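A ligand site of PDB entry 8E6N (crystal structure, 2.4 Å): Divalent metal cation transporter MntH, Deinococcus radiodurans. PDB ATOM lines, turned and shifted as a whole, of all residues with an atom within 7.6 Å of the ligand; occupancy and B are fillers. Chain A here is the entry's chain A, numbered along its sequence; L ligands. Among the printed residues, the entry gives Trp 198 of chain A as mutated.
Residues that only touch the ligand: Leu 195 (3.9 Å), Trp 198 (3.2 Å), Gly 270 (3.6 Å) and Ser 346 (3.4 Å).
The nearest printed residue that does not touch the ligand is Ala 36 (4.2 Å).
OE1 of Glu 40 lies within salt-bridge range of N2 of the ligand, 3.1 Å away.
N1 of the ligand sits at hydrogen-bond distance from OD1 of Asn 268, 2.7 Å away.
The side-chain carboxylate (OE2) of Glu 40 is in salt-bridge range of the guanidinium group (NH1) of Arg 44 (2.9 Å).
The backbone NH of Ser 346 sits at hydrogen-bond distance from the side-chain carboxylate of Asp 344 (2.7 Å).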
ATOM      1  N   GLY A  33      -9.660  11.893  26.489  1.00  0.00           N
ATOM      2  CA  GLY A  33      -9.169  12.331  25.189  1.00  0.00           C
ATOM      3  C   GLY A  33      -9.231  11.240  24.137  1.00  0.00           C
ATOM      4  O   GLY A  33      -9.559  11.496  22.976  1.00  0.00           O
ATOM      5  N   ALA A  36     -13.020  10.499  22.704  1.00  0.00           N
ATOM      6  CA  ALA A  36     -13.533  11.337  21.627  1.00  0.00           C
ATOM      7  C   ALA A  36     -12.915  10.958  20.284  1.00  0.00           C
ATOM      8  O   ALA A  36     -13.590  11.012  19.249  1.00  0.00           O
ATOM      9  CB  ALA A  36     -13.273  12.804  21.935  1.00  0.00           C
ATOM     10  N   THR A  37     -11.639  10.566  20.278  1.00  0.00           N
ATOM     11  CA  THR A  37     -10.980  10.227  19.031  1.00  0.00           C
ATOM     12  C   THR A  37     -11.456   8.876  18.496  1.00  0.00           C
ATOM     13  O   THR A  37     -11.740   8.738  17.300  1.00  0.00           O
ATOM     14  CB  THR A  37      -9.460  10.213  19.224  1.00  0.00           C
ATOM     15  OG1 THR A  37      -9.037  11.460  19.776  1.00  0.00           O
ATOM     16  CG2 THR A  37      -8.763  10.005  17.882  1.00  0.00           C
ATOM     17  N   ASN A  38     -11.557   7.878  19.376  1.00  0.00           N
ATOM     18  CA  ASN A  38     -11.933   6.541  18.932  1.00  0.00           C
ATOM     19  C   ASN A  38     -13.383   6.499  18.444  1.00  0.00           C
ATOM     20  O   ASN A  38     -13.699   5.781  17.486  1.00  0.00           O
ATOM     21  CB  ASN A  38     -11.729   5.541  20.068  1.00  0.00           C
ATOM     22  CG  ASN A  38     -10.289   5.486  20.544  1.00  0.00           C
ATOM     23  OD1 ASN A  38      -9.374   5.883  19.829  1.00  0.00           O
ATOM     24  ND2 ASN A  38     -10.088   4.992  21.759  1.00  0.00           N
ATOM     25  N   ILE A  39     -14.277   7.272  19.075  1.00  0.00           N
ATOM     26  CA  ILE A  39     -15.670   7.274  18.643  1.00  0.00           C
ATOM     27  C   ILE A  39     -15.808   7.943  17.286  1.00  0.00           C
ATOM     28  O   ILE A  39     -16.555   7.475  16.418  1.00  0.00           O
ATOM     29  CB  ILE A  39     -16.546   7.967  19.712  1.00  0.00           C
ATOM     30  CG1 ILE A  39     -16.593   7.106  20.980  1.00  0.00           C
ATOM     31  CG2 ILE A  39     -17.939   8.197  19.176  1.00  0.00           C
ATOM     32  CD1 ILE A  39     -17.444   7.706  22.076  1.00  0.00           C
ATOM     33  N   GLU A  40     -15.089   9.050  17.068  1.00  0.00           N
ATOM     34  CA  GLU A  40     -15.176   9.761  15.796  1.00  0.00           C
ATOM     35  C   GLU A  40     -14.653   8.907  14.650  1.00  0.00           C
ATOM     36  O   GLU A  40     -15.195   8.927  13.547  1.00  0.00           O
ATOM     37  CB  GLU A  40     -14.413  11.082  15.874  1.00  0.00           C
ATOM     38  CG  GLU A  40     -14.549  11.950  14.648  1.00  0.00           C
ATOM     39  CD  GLU A  40     -13.442  12.981  14.534  1.00  0.00           C
ATOM     40  OE1 GLU A  40     -12.384  12.766  15.166  1.00  0.00           O
ATOM     41  OE2 GLU A  40     -13.631  13.994  13.831  1.00  0.00           O
ATOM     42  N   GLY A  41     -13.574   8.145  14.899  1.00  0.00           N
ATOM     43  CA  GLY A  41     -13.028   7.304  13.852  1.00  0.00           C
ATOM     44  C   GLY A  41     -13.953   6.171  13.444  1.00  0.00           C
ATOM     45  O   GLY A  41     -13.962   5.763  12.283  1.00  0.00           O
ATOM     46  N   ARG A  44     -17.301   7.668  11.302  1.00  0.00           N
ATOM     47  CA  ARG A  44     -17.024   8.258  10.006  1.00  0.00           C
ATOM     48  C   ARG A  44     -16.378   7.277   9.024  1.00  0.00           C
ATOM     49  O   ARG A  44     -16.608   7.385   7.817  1.00  0.00           O
ATOM     50  CB  ARG A  44     -16.135   9.485  10.159  1.00  0.00           C
ATOM     51  CG  ARG A  44     -16.743  10.578  11.021  1.00  0.00           C
ATOM     52  CD  ARG A  44     -15.780  11.740  11.227  1.00  0.00           C
ATOM     53  NE  ARG A  44     -15.464  12.413   9.970  1.00  0.00           N
ATOM     54  CZ  ARG A  44     -14.655  13.451   9.874  1.00  0.00           C
ATOM     55  NH1 ARG A  44     -14.058  13.969  10.935  1.00  0.00           N
ATOM     56  NH2 ARG A  44     -14.436  13.992   8.673  1.00  0.00           N
ATOM     57  N   TYR A 194      -5.948  12.302   7.879  1.00  0.00           N
ATOM     58  CA  TYR A 194      -5.724  13.274   8.944  1.00  0.00           C
ATOM     59  C   TYR A 194      -6.054  12.695  10.307  1.00  0.00           C
ATOM     60  O   TYR A 194      -5.337  12.931  11.285  1.00  0.00           O
ATOM     61  CB  TYR A 194      -6.566  14.530   8.675  1.00  0.00           C
ATOM     62  CG  TYR A 194      -6.427  15.605   9.734  1.00  0.00           C
ATOM     63  CD1 TYR A 194      -5.366  16.509   9.692  1.00  0.00           C
ATOM     64  CD2 TYR A 194      -7.346  15.720  10.756  1.00  0.00           C
ATOM     65  CE1 TYR A 194      -5.233  17.482  10.656  1.00  0.00           C
ATOM     66  CE2 TYR A 194      -7.225  16.701  11.721  1.00  0.00           C
ATOM     67  CZ  TYR A 194      -6.162  17.585  11.671  1.00  0.00           C
ATOM     68  OH  TYR A 194      -6.034  18.567  12.625  1.00  0.00           O
ATOM     69  N   LEU A 195      -7.136  11.923  10.402  1.00  0.00           N
ATOM     70  CA  LEU A 195      -7.542  11.363  11.683  1.00  0.00           C
ATOM     71  C   LEU A 195      -6.563  10.308  12.171  1.00  0.00           C
ATOM     72  O   LEU A 195      -6.366  10.153  13.378  1.00  0.00           O
ATOM     73  CB  LEU A 195      -8.944  10.779  11.581  1.00  0.00           C
ATOM     74  CG  LEU A 195      -9.588  10.299  12.882  1.00  0.00           C
ATOM     75  CD1 LEU A 195      -9.473  11.374  13.958  1.00  0.00           C
ATOM     76  CD2 LEU A 195     -11.039   9.953  12.644  1.00  0.00           C
ATOM     77  N   ALA A 196      -5.923   9.564  11.250  1.00  0.00           N
ATOM     78  CA  ALA A 196      -4.927   8.581  11.659  1.00  0.00           C
ATOM     79  C   ALA A 196      -3.674   9.269  12.194  1.00  0.00           C
ATOM     80  O   ALA A 196      -3.115   8.850  13.208  1.00  0.00           O
ATOM     81  CB  ALA A 196      -4.579   7.670  10.488  1.00  0.00           C
ATOM     82  N   TRP A 198      -3.545  12.100  13.597  1.00  0.00           N
ATOM     83  CA  TRP A 198      -3.873  12.699  14.889  1.00  0.00           C
ATOM     84  C   TRP A 198      -3.790  11.677  16.021  1.00  0.00           C
ATOM     85  O   TRP A 198      -3.543  12.054  17.175  1.00  0.00           O
ATOM     86  CB  TRP A 198      -5.263  13.334  14.827  1.00  0.00           C
ATOM     87  CG  TRP A 198      -5.435  14.487  15.756  1.00  0.00           C
ATOM     88  CD1 TRP A 198      -5.080  15.784  15.524  1.00  0.00           C
ATOM     89  CD2 TRP A 198      -6.025  14.459  17.068  1.00  0.00           C
ATOM     90  NE1 TRP A 198      -5.405  16.561  16.601  1.00  0.00           N
ATOM     91  CE2 TRP A 198      -5.989  15.774  17.567  1.00  0.00           C
ATOM     92  CE3 TRP A 198      -6.583  13.449  17.851  1.00  0.00           C
ATOM     93  CZ2 TRP A 198      -6.476  16.108  18.824  1.00  0.00           C
ATOM     94  CZ3 TRP A 198      -7.070  13.783  19.109  1.00  0.00           C
ATOM     95  CH2 TRP A 198      -7.014  15.107  19.580  1.00  0.00           C
ATOM     96  N   ILE A 199      -3.994  10.397  15.719  1.00  0.00           N
ATOM     97  CA  ILE A 199      -3.916   9.374  16.745  1.00  0.00           C
ATOM     98  C   ILE A 199      -2.467   9.126  17.149  1.00  0.00           C
ATOM     99  O   ILE A 199      -2.128   9.159  18.341  1.00  0.00           O
ATOM    100  CB  ILE A 199      -4.592   8.068  16.253  1.00  0.00           C
ATOM    101  CG1 ILE A 199      -6.086   8.284  16.022  1.00  0.00           C
ATOM    102  CG2 ILE A 199      -4.358   6.940  17.249  1.00  0.00           C
ATOM    103  CD1 ILE A 199      -6.811   7.054  15.536  1.00  0.00           C
ATOM    104  N   GLU A 267     -23.665  12.424  12.040  1.00  0.00           N
ATOM    105  CA  GLU A 267     -22.730  13.541  12.014  1.00  0.00           C
ATOM    106  C   GLU A 267     -22.378  13.966  13.433  1.00  0.00           C
ATOM    107  O   GLU A 267     -23.114  13.727  14.384  1.00  0.00           O
ATOM    108  CB  GLU A 267     -23.328  14.727  11.250  1.00  0.00           C
ATOM    109  CG  GLU A 267     -23.661  14.419   9.799  1.00  0.00           C
ATOM    110  CD  GLU A 267     -24.340  15.592   9.100  1.00  0.00           C
ATOM    111  OE1 GLU A 267     -24.583  16.621   9.764  1.00  0.00           O
ATOM    112  OE2 GLU A 267     -24.638  15.470   7.894  1.00  0.00           O
ATOM    113  N   ASN A 268     -21.208  14.600  13.556  1.00  0.00           N
ATOM    114  CA  ASN A 268     -20.670  15.082  14.829  1.00  0.00           C
ATOM    115  C   ASN A 268     -20.533  13.929  15.819  1.00  0.00           C
ATOM    116  O   ASN A 268     -21.275  13.789  16.790  1.00  0.00           O
ATOM    117  CB  ASN A 268     -21.552  16.213  15.397  1.00  0.00           C
ATOM    118  CG  ASN A 268     -20.812  17.091  16.378  1.00  0.00           C
ATOM    119  OD1 ASN A 268     -19.601  16.937  16.581  1.00  0.00           O
ATOM    120  ND2 ASN A 268     -21.522  18.025  16.995  1.00  0.00           N
ATOM    121  N   ALA A 269     -19.535  13.080  15.530  1.00  0.00           N
ATOM    122  CA  ALA A 269     -19.308  11.873  16.305  1.00  0.00           C
ATOM    123  C   ALA A 269     -18.288  12.067  17.418  1.00  0.00           C
ATOM    124  O   ALA A 269     -18.359  11.376  18.436  1.00  0.00           O
ATOM    125  CB  ALA A 269     -18.855  10.732  15.391  1.00  0.00           C
ATOM    126  N   GLY A 270     -17.325  12.971  17.229  1.00  0.00           N
ATOM    127  CA  GLY A 270     -16.315  13.192  18.252  1.00  0.00           C
ATOM    128  C   GLY A 270     -16.889  13.699  19.565  1.00  0.00           C
ATOM    129  O   GLY A 270     -16.349  13.426  20.634  1.00  0.00           O
ATOM    130  N   ASP A 271     -17.989  14.448  19.495  1.00  0.00           N
ATOM    131  CA  ASP A 271     -18.654  14.923  20.696  1.00  0.00           C
ATOM    132  C   ASP A 271     -19.273  13.739  21.430  1.00  0.00           C
ATOM    133  O   ASP A 271     -20.085  13.002  20.867  1.00  0.00           O
ATOM    134  CB  ASP A 271     -19.728  15.955  20.348  1.00  0.00           C
ATOM    135  CG  ASP A 271     -20.256  16.679  21.560  1.00  0.00           C
ATOM    136  OD1 ASP A 271     -19.712  16.480  22.661  1.00  0.00           O
ATOM    137  OD2 ASP A 271     -21.230  17.460  21.414  1.00  0.00           O
ATOM    138  N   LEU A 272     -18.887  13.557  22.691  1.00  0.00           N
ATOM    139  CA  LEU A 272     -19.383  12.426  23.474  1.00  0.00           C
ATOM    140  C   LEU A 272     -20.863  12.534  23.794  1.00  0.00           C
ATOM    141  O   LEU A 272     -21.469  11.530  24.184  1.00  0.00           O
ATOM    142  CB  LEU A 272     -18.568  12.290  24.755  1.00  0.00           C
ATOM    143  CG  LEU A 272     -17.054  12.152  24.582  1.00  0.00           C
ATOM    144  CD1 LEU A 272     -16.342  12.191  25.924  1.00  0.00           C
ATOM    145  CD2 LEU A 272     -16.717  10.880  23.829  1.00  0.00           C
ATOM    146  N   ASP A 344     -15.481  25.925  22.670  1.00  0.00           N
ATOM    147  CA  ASP A 344     -15.845  24.788  21.833  1.00  0.00           C
ATOM    148  C   ASP A 344     -15.026  23.559  22.240  1.00  0.00           C
ATOM    149  O   ASP A 344     -13.827  23.671  22.502  1.00  0.00           O
ATOM    150  CB  ASP A 344     -15.598  25.124  20.359  1.00  0.00           C
ATOM    151  CG  ASP A 344     -16.242  24.116  19.415  1.00  0.00           C
ATOM    152  OD1 ASP A 344     -15.858  22.926  19.441  1.00  0.00           O
ATOM    153  OD2 ASP A 344     -17.120  24.525  18.634  1.00  0.00           O
ATOM    154  N   PRO A 345     -15.651  22.388  22.329  1.00  0.00           N
ATOM    155  CA  PRO A 345     -14.892  21.175  22.664  1.00  0.00           C
ATOM    156  C   PRO A 345     -13.772  20.868  21.684  1.00  0.00           C
ATOM    157  O   PRO A 345     -12.766  20.260  22.073  1.00  0.00           O
ATOM    158  CB  PRO A 345     -15.963  20.070  22.662  1.00  0.00           C
ATOM    159  CG  PRO A 345     -17.237  20.793  22.933  1.00  0.00           C
ATOM    160  CD  PRO A 345     -17.101  22.133  22.267  1.00  0.00           C
ATOM    161  N   SER A 346     -13.923  21.269  20.420  1.00  0.00           N
ATOM    162  CA  SER A 346     -12.850  21.066  19.450  1.00  0.00           C
ATOM    163  C   SER A 346     -11.758  22.117  19.573  1.00  0.00           C
ATOM    164  O   SER A 346     -10.603  21.858  19.193  1.00  0.00           O
ATOM    165  CB  SER A 346     -13.415  21.050  18.035  1.00  0.00           C
ATOM    166  OG  SER A 346     -14.332  19.972  17.856  1.00  0.00           O
ATOM    167  N   LEU A 349      -9.333  21.020  22.432  1.00  0.00           N
ATOM    168  CA  LEU A 349      -8.498  19.879  22.087  1.00  0.00           C
ATOM    169  C   LEU A 349      -7.368  20.241  21.137  1.00  0.00           C
ATOM    170  O   LEU A 349      -6.411  19.475  21.012  1.00  0.00           O
ATOM    171  CB  LEU A 349      -9.354  18.776  21.447  1.00  0.00           C
ATOM    172  CG  LEU A 349     -10.360  18.069  22.364  1.00  0.00           C
ATOM    173  CD1 LEU A 349     -11.102  16.976  21.605  1.00  0.00           C
ATOM    174  CD2 LEU A 349      -9.665  17.493  23.590  1.00  0.00           C
ATOM    175  N   ILE A 350      -7.451  21.395  20.478  1.00  0.00           N
ATOM    176  CA  ILE A 350      -6.371  21.833  19.593  1.00  0.00           C
ATOM    177  C   ILE A 350      -5.291  22.548  20.388  1.00  0.00           C
ATOM    178  O   ILE A 350      -4.095  22.327  20.180  1.00  0.00           O
ATOM    179  CB  ILE A 350      -6.921  22.705  18.452  1.00  0.00           C
ATOM    180  CG1 ILE A 350      -7.166  21.860  17.195  1.00  0.00           C
ATOM    181  CG2 ILE A 350      -5.984  23.865  18.135  1.00  0.00           C
ATOM    182  CD1 ILE A 350      -8.156  20.737  17.380  1.00  0.00           C
HETATM  183  N1  LIG L   1     -16.936  17.090  15.932  1.00  0.00           N
HETATM  184  C1  LIG L   1     -15.722  16.978  15.143  1.00  0.00           C
HETATM  185  C2  LIG L   1     -14.509  17.147  16.059  1.00  0.00           C
HETATM  186  C3  LIG L   1     -14.662  16.233  17.272  1.00  0.00           C
HETATM  187  C4  LIG L   1     -13.301  16.066  17.952  1.00  0.00           C
HETATM  188  N2  LIG L   1     -12.704  14.801  17.546  1.00  0.00           N
HETATM  189  C5  LIG L   1     -11.301  15.006  17.253  1.00  0.00           C
HETATM  190  C6  LIG L   1     -11.160  15.676  15.892  1.00  0.00           C
HETATM  191  C7  LIG L   1      -9.690  15.972  15.615  1.00  0.00           C
HETATM  192  N3  LIG L   1      -8.919  14.758  15.780  1.00  0.00           N
